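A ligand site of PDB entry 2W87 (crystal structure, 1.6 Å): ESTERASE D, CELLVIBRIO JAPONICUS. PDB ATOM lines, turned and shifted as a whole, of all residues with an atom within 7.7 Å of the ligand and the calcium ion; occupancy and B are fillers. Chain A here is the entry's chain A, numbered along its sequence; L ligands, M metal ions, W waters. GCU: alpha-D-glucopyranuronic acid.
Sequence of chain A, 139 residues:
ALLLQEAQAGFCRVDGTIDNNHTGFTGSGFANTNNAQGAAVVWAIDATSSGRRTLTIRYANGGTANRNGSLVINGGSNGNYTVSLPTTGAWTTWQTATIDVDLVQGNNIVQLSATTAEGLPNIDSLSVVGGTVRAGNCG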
ATOM      1  N   ASP A  15      15.237 -37.312 -12.027  1.00  0.00           N
ATOM      2  CA  ASP A  15      16.571 -37.882 -12.084  1.00  0.00           C
ATOM      3  C   ASP A  15      17.471 -36.996 -11.249  1.00  0.00           C
ATOM      4  O   ASP A  15      18.054 -36.033 -11.745  1.00  0.00           O
ATOM      5  CB  ASP A  15      17.065 -37.951 -13.520  1.00  0.00           C
ATOM      6  CG  ASP A  15      16.169 -38.788 -14.397  1.00  0.00           C
ATOM      7  OD1 ASP A  15      15.744 -39.885 -13.904  1.00  0.00           O
ATOM      8  OD2 ASP A  15      15.848 -38.338 -15.544  1.00  0.00           O
ATOM      9  N   GLY A  16      17.541 -37.320  -9.968  1.00  0.00           N
ATOM     10  CA  GLY A  16      18.118 -36.412  -8.974  1.00  0.00           C
ATOM     11  C   GLY A  16      17.403 -36.589  -7.648  1.00  0.00           C
ATOM     12  O   GLY A  16      17.078 -37.699  -7.257  1.00  0.00           O
ATOM     13  N   THR A  17      17.113 -35.493  -6.950  1.00  0.00           N
ATOM     14  CA  THR A  17      16.481 -35.556  -5.646  1.00  0.00           C
ATOM     15  C   THR A  17      15.379 -34.536  -5.534  1.00  0.00           C
ATOM     16  O   THR A  17      15.332 -33.597  -6.311  1.00  0.00           O
ATOM     17  CB  THR A  17      17.500 -35.291  -4.501  1.00  0.00           C
ATOM     18  OG1 THR A  17      18.261 -34.099  -4.750  1.00  0.00           O
ATOM     19  CG2 THR A  17      18.443 -36.469  -4.317  1.00  0.00           C
ATOM     20  N   ASP A  19      14.478 -31.724  -2.948  1.00  0.00           N
ATOM     21  CA  ASP A  19      15.228 -30.988  -1.953  1.00  0.00           C
ATOM     22  C   ASP A  19      14.382 -29.847  -1.409  1.00  0.00           C
ATOM     23  O   ASP A  19      13.327 -29.486  -1.968  1.00  0.00           O
ATOM     24  CB  ASP A  19      16.503 -30.388  -2.560  1.00  0.00           C
ATOM     25  CG  ASP A  19      17.512 -31.409  -2.983  1.00  0.00           C
ATOM     26  OD1 ASP A  19      17.279 -32.628  -2.835  1.00  0.00           O
ATOM     27  OD2 ASP A  19      18.580 -30.964  -3.455  1.00  0.00           O
ATOM     28  N   ASN A  21      16.405 -27.225   0.673  1.00  0.00           N
ATOM     29  CA  ASN A  21      17.468 -26.479   1.370  1.00  0.00           C
ATOM     30  C   ASN A  21      17.734 -25.069   0.821  1.00  0.00           C
ATOM     31  O   ASN A  21      18.752 -24.455   1.155  1.00  0.00           O
ATOM     32  CB  ASN A  21      18.766 -27.285   1.337  1.00  0.00           C
ATOM     33  CG  ASN A  21      19.304 -27.476  -0.067  1.00  0.00           C
ATOM     34  OD1 ASN A  21      18.531 -27.575  -1.013  1.00  0.00           O
ATOM     35  ND2 ASN A  21      20.621 -27.500  -0.219  1.00  0.00           N
ATOM     36  N   HIS A  22      16.856 -24.582  -0.038  1.00  0.00           N
ATOM     37  CA  HIS A  22      16.863 -23.183  -0.435  1.00  0.00           C
ATOM     38  C   HIS A  22      15.456 -22.661  -0.258  1.00  0.00           C
ATOM     39  O   HIS A  22      14.512 -23.312  -0.672  1.00  0.00           O
ATOM     40  CB  HIS A  22      17.234 -23.031  -1.916  1.00  0.00           C
ATOM     41  CG  HIS A  22      18.589 -23.549  -2.272  1.00  0.00           C
ATOM     42  ND1 HIS A  22      19.748 -23.017  -1.736  1.00  0.00           N
ATOM     43  CD2 HIS A  22      18.979 -24.508  -3.142  1.00  0.00           C
ATOM     44  CE1 HIS A  22      20.783 -23.651  -2.258  1.00  0.00           C
ATOM     45  NE2 HIS A  22      20.346 -24.564  -3.098  1.00  0.00           N
ATOM     46  N   PHE A  30      11.420 -28.890  -3.969  1.00  0.00           N
ATOM     47  CA  PHE A  30      11.654 -28.671  -5.393  1.00  0.00           C
ATOM     48  C   PHE A  30      12.462 -29.834  -5.936  1.00  0.00           C
ATOM     49  O   PHE A  30      13.136 -30.534  -5.190  1.00  0.00           O
ATOM     50  CB  PHE A  30      12.388 -27.352  -5.612  1.00  0.00           C
ATOM     51  CG  PHE A  30      13.635 -27.184  -4.784  1.00  0.00           C
ATOM     52  CD1 PHE A  30      14.849 -27.695  -5.217  1.00  0.00           C
ATOM     53  CD2 PHE A  30      13.611 -26.491  -3.587  1.00  0.00           C
ATOM     54  CE1 PHE A  30      15.989 -27.534  -4.473  1.00  0.00           C
ATOM     55  CE2 PHE A  30      14.754 -26.316  -2.844  1.00  0.00           C
ATOM     56  CZ  PHE A  30      15.946 -26.830  -3.279  1.00  0.00           C
ATOM     57  N   ALA A  31      12.325 -30.073  -7.234  1.00  0.00           N
ATOM     58  CA  ALA A  31      13.072 -31.150  -7.881  1.00  0.00           C
ATOM     59  C   ALA A  31      14.453 -30.597  -8.274  1.00  0.00           C
ATOM     60  O   ALA A  31      14.561 -29.582  -8.975  1.00  0.00           O
ATOM     61  CB  ALA A  31      12.319 -31.656  -9.110  1.00  0.00           C
ATOM     62  N   ASN A  32      15.494 -31.318  -7.855  1.00  0.00           N
ATOM     63  CA  ASN A  32      16.868 -30.963  -8.152  1.00  0.00           C
ATOM     64  C   ASN A  32      17.509 -32.043  -9.032  1.00  0.00           C
ATOM     65  O   ASN A  32      17.864 -33.106  -8.535  1.00  0.00           O
ATOM     66  CB  ASN A  32      17.646 -30.845  -6.841  1.00  0.00           C
ATOM     67  CG  ASN A  32      19.129 -30.605  -7.049  1.00  0.00           C
ATOM     68  OD1 ASN A  32      19.607 -30.476  -8.186  1.00  0.00           O
ATOM     69  ND2 ASN A  32      19.881 -30.561  -5.928  1.00  0.00           N
ATOM     70  N   THR A  33      17.621 -31.800 -10.325  1.00  0.00           N
ATOM     71  CA  THR A  33      18.209 -32.794 -11.229  1.00  0.00           C
ATOM     72  C   THR A  33      19.706 -32.980 -10.976  1.00  0.00           C
ATOM     73  O   THR A  33      20.415 -32.033 -10.602  1.00  0.00           O
ATOM     74  CB  THR A  33      18.068 -32.414 -12.725  1.00  0.00           C
ATOM     75  OG1 THR A  33      18.642 -31.133 -12.971  1.00  0.00           O
ATOM     76  CG2 THR A  33      16.602 -32.439 -13.144  1.00  0.00           C
ATOM     77  N   ASN A  34      20.162 -34.210 -11.177  1.00  0.00           N
ATOM     78  CA  ASN A  34      21.545 -34.479 -11.461  1.00  0.00           C
ATOM     79  C   ASN A  34      22.093 -33.445 -12.421  1.00  0.00           C
ATOM     80  O   ASN A  34      21.379 -33.001 -13.313  1.00  0.00           O
ATOM     81  CB  ASN A  34      21.678 -35.835 -12.169  1.00  0.00           C
ATOM     82  CG  ASN A  34      21.304 -37.023 -11.280  1.00  0.00           C
ATOM     83  OD1 ASN A  34      21.462 -36.962 -10.063  1.00  0.00           O
ATOM     84  ND2 ASN A  34      20.837 -38.125 -11.897  1.00  0.00           N
ATOM     85  N   ASN A  35      23.366 -33.095 -12.274  1.00  0.00           N
ATOM     86  CA  ASN A  35      24.022 -32.178 -13.192  1.00  0.00           C
ATOM     87  C   ASN A  35      24.585 -32.954 -14.384  1.00  0.00           C
ATOM     88  O   ASN A  35      25.786 -33.258 -14.449  1.00  0.00           O
ATOM     89  CB  ASN A  35      25.077 -31.378 -12.435  1.00  0.00           C
ATOM     90  CG  ASN A  35      24.527 -30.787 -11.139  1.00  0.00           C
ATOM     91  OD1 ASN A  35      23.347 -30.415 -11.072  1.00  0.00           O
ATOM     92  ND2 ASN A  35      25.348 -30.765 -10.102  1.00  0.00           N
ATOM     93  N   ALA A  36      23.697 -33.285 -15.303  1.00  0.00           N
ATOM     94  CA  ALA A  36      23.988 -34.065 -16.482  1.00  0.00           C
ATOM     95  C   ALA A  36      22.987 -33.736 -17.565  1.00  0.00           C
ATOM     96  O   ALA A  36      21.806 -33.501 -17.298  1.00  0.00           O
ATOM     97  CB  ALA A  36      23.911 -35.541 -16.154  1.00  0.00           C
ATOM     98  N   ALA A  39      19.114 -35.153 -17.813  1.00  0.00           N
ATOM     99  CA  ALA A  39      18.448 -35.340 -16.526  1.00  0.00           C
ATOM    100  C   ALA A  39      17.076 -34.644 -16.537  1.00  0.00           C
ATOM    101  O   ALA A  39      16.956 -33.488 -16.957  1.00  0.00           O
ATOM    102  CB  ALA A  39      19.326 -34.842 -15.381  1.00  0.00           C
ATOM    103  N   ALA A  60      14.315 -22.056 -10.061  1.00  0.00           N
ATOM    104  CA  ALA A  60      15.417 -21.223  -9.590  1.00  0.00           C
ATOM    105  C   ALA A  60      16.676 -21.684 -10.279  1.00  0.00           C
ATOM    106  O   ALA A  60      16.904 -22.866 -10.376  1.00  0.00           O
ATOM    107  CB  ALA A  60      15.581 -21.355  -8.086  1.00  0.00           C
ATOM    108  N   ASN A  61      17.488 -20.744 -10.750  1.00  0.00           N
ATOM    109  CA  ASN A  61      18.726 -21.066 -11.441  1.00  0.00           C
ATOM    110  C   ASN A  61      19.791 -20.124 -10.903  1.00  0.00           C
ATOM    111  O   ASN A  61      19.899 -19.008 -11.374  1.00  0.00           O
ATOM    112  CB  ASN A  61      18.554 -20.918 -12.949  1.00  0.00           C
ATOM    113  CG  ASN A  61      19.806 -21.237 -13.718  1.00  0.00           C
ATOM    114  OD1 ASN A  61      20.867 -21.505 -13.143  1.00  0.00           O
ATOM    115  ND2 ASN A  61      19.703 -21.195 -15.046  1.00  0.00           N
ATOM    116  N   GLY A  62      20.549 -20.594  -9.920  1.00  0.00           N
ATOM    117  CA  GLY A  62      21.617 -19.814  -9.295  1.00  0.00           C
ATOM    118  C   GLY A  62      22.961 -20.046  -9.971  1.00  0.00           C
ATOM    119  O   GLY A  62      24.009 -19.625  -9.473  1.00  0.00           O
ATOM    120  N   GLY A  63      22.930 -20.728 -11.115  1.00  0.00           N
ATOM    121  CA  GLY A  63      24.145 -20.955 -11.895  1.00  0.00           C
ATOM    122  C   GLY A  63      24.424 -19.736 -12.736  1.00  0.00           C
ATOM    123  O   GLY A  63      23.700 -18.744 -12.635  1.00  0.00           O
ATOM    124  N   ARG A  67      19.992 -22.922 -18.383  1.00  0.00           N
ATOM    125  CA  ARG A  67      19.913 -24.363 -18.308  1.00  0.00           C
ATOM    126  C   ARG A  67      18.620 -24.778 -19.022  1.00  0.00           C
ATOM    127  O   ARG A  67      17.680 -25.319 -18.400  1.00  0.00           O
ATOM    128  CB  ARG A  67      19.917 -24.772 -16.861  1.00  0.00           C
ATOM    129  CG  ARG A  67      21.195 -24.513 -16.168  1.00  0.00           C
ATOM    130  CD  ARG A  67      21.149 -25.117 -14.801  1.00  0.00           C
ATOM    131  NE  ARG A  67      22.365 -24.839 -14.037  1.00  0.00           N
ATOM    132  CZ  ARG A  67      22.678 -25.460 -12.906  1.00  0.00           C
ATOM    133  NH1 ARG A  67      21.875 -26.386 -12.401  1.00  0.00           N
ATOM    134  NH2 ARG A  67      23.807 -25.149 -12.283  1.00  0.00           N
ATOM    135  N   TRP A  91      19.852 -19.303  -5.949  1.00  0.00           N
ATOM    136  CA  TRP A  91      19.040 -20.495  -5.761  1.00  0.00           C
ATOM    137  C   TRP A  91      17.784 -20.230  -4.926  1.00  0.00           C
ATOM    138  O   TRP A  91      16.884 -21.066  -4.813  1.00  0.00           O
ATOM    139  CB  TRP A  91      19.857 -21.639  -5.139  1.00  0.00           C
ATOM    140  CG  TRP A  91      20.939 -22.098  -6.023  1.00  0.00           C
ATOM    141  CD1 TRP A  91      22.283 -21.910  -5.867  1.00  0.00           C
ATOM    142  CD2 TRP A  91      20.780 -22.783  -7.277  1.00  0.00           C
ATOM    143  NE1 TRP A  91      22.972 -22.451  -6.914  1.00  0.00           N
ATOM    144  CE2 TRP A  91      22.072 -23.002  -7.807  1.00  0.00           C
ATOM    145  CE3 TRP A  91      19.683 -23.253  -8.001  1.00  0.00           C
ATOM    146  CZ2 TRP A  91      22.298 -23.650  -9.020  1.00  0.00           C
ATOM    147  CZ3 TRP A  91      19.900 -23.900  -9.218  1.00  0.00           C
ATOM    148  CH2 TRP A  91      21.192 -24.103  -9.719  1.00  0.00           C
ATOM    149  N   GLU A 118      24.906 -29.119 -17.197  1.00  0.00           N
ATOM    150  CA  GLU A 118      24.613 -28.627 -15.842  1.00  0.00           C
ATOM    151  C   GLU A 118      23.295 -29.186 -15.297  1.00  0.00           C
ATOM    152  O   GLU A 118      23.000 -29.029 -14.125  1.00  0.00           O
ATOM    153  CB  GLU A 118      24.527 -27.106 -15.819  1.00  0.00           C
ATOM    154  CG  GLU A 118      25.822 -26.392 -16.112  1.00  0.00           C
ATOM    155  CD  GLU A 118      25.794 -24.945 -15.630  1.00  0.00           C
ATOM    156  OE1 GLU A 118      25.893 -24.724 -14.401  1.00  0.00           O
ATOM    157  OE2 GLU A 118      25.726 -24.042 -16.497  1.00  0.00           O
ATOM    158  N   GLY A 119      22.534 -29.859 -16.148  1.00  0.00           N
ATOM    159  CA  GLY A 119      21.230 -30.338 -15.730  1.00  0.00           C
ATOM    160  C   GLY A 119      20.227 -29.197 -15.819  1.00  0.00           C
ATOM    161  O   GLY A 119      20.464 -28.181 -16.488  1.00  0.00           O
ATOM    162  N   LEU A 120      19.084 -29.365 -15.161  1.00  0.00           N
ATOM    163  CA  LEU A 120      18.076 -28.327 -15.127  1.00  0.00           C
ATOM    164  C   LEU A 120      18.303 -27.334 -13.991  1.00  0.00           C
ATOM    165  O   LEU A 120      19.093 -27.568 -13.096  1.00  0.00           O
ATOM    166  CB  LEU A 120      16.691 -28.965 -14.952  1.00  0.00           C
ATOM    167  CG  LEU A 120      16.136 -29.733 -16.145  1.00  0.00           C
ATOM    168  CD1 LEU A 120      14.783 -30.412 -15.735  1.00  0.00           C
ATOM    169  CD2 LEU A 120      15.921 -28.815 -17.341  1.00  0.00           C
ATOM    170  N   PRO A 121      17.559 -26.213 -14.021  1.00  0.00           N
ATOM    171  CA  PRO A 121      17.463 -25.457 -12.793  1.00  0.00           C
ATOM    172  C   PRO A 121      16.712 -26.304 -11.762  1.00  0.00           C
ATOM    173  O   PRO A 121      16.235 -27.410 -12.088  1.00  0.00           O
ATOM    174  CB  PRO A 121      16.617 -24.258 -13.184  1.00  0.00           C
ATOM    175  CG  PRO A 121      16.485 -24.272 -14.612  1.00  0.00           C
ATOM    176  CD  PRO A 121      16.704 -25.672 -15.085  1.00  0.00           C
ATOM    177  N   ASN A 122      16.618 -25.814 -10.528  1.00  0.00           N
ATOM    178  CA  ASN A 122      15.737 -26.447  -9.553  1.00  0.00           C
ATOM    179  C   ASN A 122      14.293 -26.116  -9.923  1.00  0.00           C
ATOM    180  O   ASN A 122      13.981 -24.953 -10.210  1.00  0.00           O
ATOM    181  CB  ASN A 122      16.069 -25.937  -8.152  1.00  0.00           C
ATOM    182  CG  ASN A 122      17.402 -26.460  -7.626  1.00  0.00           C
ATOM    183  OD1 ASN A 122      17.909 -27.512  -8.078  1.00  0.00           O
ATOM    184  ND2 ASN A 122      17.962 -25.778  -6.646  1.00  0.00           N
ATOM    185  N   ILE A 123      13.422 -27.110  -9.928  1.00  0.00           N
ATOM    186  CA  ILE A 123      12.039 -26.943 -10.416  1.00  0.00           C
ATOM    187  C   ILE A 123      11.061 -27.046  -9.267  1.00  0.00           C
ATOM    188  O   ILE A 123      10.917 -28.086  -8.641  1.00  0.00           O
ATOM    189  CB  ILE A 123      11.669 -28.011 -11.482  1.00  0.00           C
ATOM    190  CG1 ILE A 123      12.717 -28.042 -12.611  1.00  0.00           C
ATOM    191  CG2 ILE A 123      10.217 -27.846 -11.939  1.00  0.00           C
ATOM    192  CD1 ILE A 123      12.861 -26.763 -13.401  1.00  0.00           C
HETATM  193  C1  GCU L   1      24.014 -26.366  -5.822  1.00  0.00           C
HETATM  194  C2  GCU L   1      22.604 -26.014  -5.327  1.00  0.00           C
HETATM  195  C3  GCU L   1      21.616 -27.055  -5.851  1.00  0.00           C
HETATM  196  C4  GCU L   1      21.643 -27.005  -7.363  1.00  0.00           C
HETATM  197  C5  GCU L   1      23.078 -27.267  -7.834  1.00  0.00           C
HETATM  198  C6  GCU L   1      23.221 -27.179  -9.346  1.00  0.00           C
HETATM  199  O1  GCU L   1      24.307 -27.670  -5.320  1.00  0.00           O
HETATM  200  O2  GCU L   1      22.591 -26.027  -3.905  1.00  0.00           O
HETATM  201  O3  GCU L   1      20.294 -26.797  -5.362  1.00  0.00           O
HETATM  202  O4  GCU L   1      20.776 -28.011  -7.947  1.00  0.00           O
HETATM  203  O5  GCU L   1      23.960 -26.293  -7.272  1.00  0.00           O
HETATM  204  O6A GCU L   1      22.382 -27.811 -10.011  1.00  0.00           O
HETATM  205  O6B GCU L   1      24.148 -26.496  -9.842  1.00  0.00           O
HETATM  206 CA    CA M   1      21.084 -29.850  -9.893  1.00  0.00          CA
HETATM  207  O   HOH W   1      19.424 -28.407  -3.397  1.00  0.00           O
HETATM  208  O   HOH W   2      22.545 -28.521  -2.692  1.00  0.00           O
HETATM  209  O   HOH W   3      26.254 -25.243  -8.705  1.00  0.00           O
HETATM  210  O   HOH W   4      22.839 -30.545  -5.601  1.00  0.00           O
HETATM  211  O   HOH W   5      18.969 -28.702 -10.461  1.00  0.00           O
HETATM  212  O   HOH W   6      22.641 -31.028  -8.442  1.00  0.00           O
HETATM  213  O   HOH W   7      20.957 -29.472 -12.328  1.00  0.00           O
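O2 of the ligand is in hydrogen-bond range of NE2 of His 22, 2.8 Å away. ND2 of Asn 122 lies within hydrogen-bond range of O3 of the ligand (2.9 Å). The guanidinium group (NH2) of Arg 67 lies within salt-bridge range of an oxygen (O6B) of the ligand.
The backbone carbonyl oxygen of Thr 17 sits at hydrogen-bond distance from the backbone NH of Asn 32 (2.8 Å). The side-chain carboxylate (OD2) of Asp 19 is in hydrogen-bond range of the side-chain amide nitrogen (ND2) of Asn 32 (2.8 Å). NH1 of Arg 67 is in hydrogen-bond range of O of Leu 120, at 3.1 Å. N of Leu 120 lies within hydrogen-bond range of OG1 of Thr 33, 2.8 Å away. The backbone carbonyl oxygen of Asn 122 lies within hydrogen-bond range of the backbone NH of Ala 60, at 2.9 Å. The side-chain amide oxygen of Asn 122 sits close to the side-chain amide oxygen of Asn 32 (3.4 Å). The side-chain amide oxygen (OD1) of Asn 35 lies close to the backbone carbonyl oxygen (O) of Glu 118, 3.4 Å away. The guanidinium group (NH2) of Arg 67 is in salt-bridge range of the side-chain carboxylate (OE1) of Glu 118, at 3.0 Å.
Trp 91 touches the ligand. Hydrophobic or aromatic side chains within 4 Å of the ligand: His 22 and Trp 91. Within 4 Å of the ligand: His 22, Asn 32, Asn 35, Arg 67, Trp 91 and Asn 122.
Three residues have an atom within 4 Å of the calcium ion: Asn 32, Thr 33 and Asn 35. The nearest printed residue that does not touch the calcium ion is Asn 122 (4.3 Å).
The calcium ion is bound by the side-chain amide oxygen of Asn 32, the backbone carbonyl oxygen of Thr 33, an oxygen (O6A) of the ligand, water W6, water W7, water W5, the side-chain amide oxygen of Asn 35 and an oxygen (O4) of the ligand. The calcium ion has eight donor atoms within binding distance.
Water W7 lies within hydrogen-bond range of the backbone carbonyl oxygen of Glu 118 (2.8 Å), the backbone carbonyl oxygen of Leu 120 (2.8 Å), the side-chain hydroxyl of Thr 33 (2.9 Å) and the guanidinium group of Arg 67 (3.2 Å). Water W1 lies within hydrogen-bond range of the side-chain amide oxygen of Asn 21 (2.7 Å), an oxygen (O3) of the ligand (2.7 Å), the side-chain carboxylate of Asp 19 (2.7 Å) and the side-chain amide nitrogen of Asn 32 (3.4 Å). Water W2 bridges O2 of the ligand and ND2 of Asn 21. Water W4 lies within hydrogen-bond range of ND2 of Asn 32 and O1 of the ligand.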
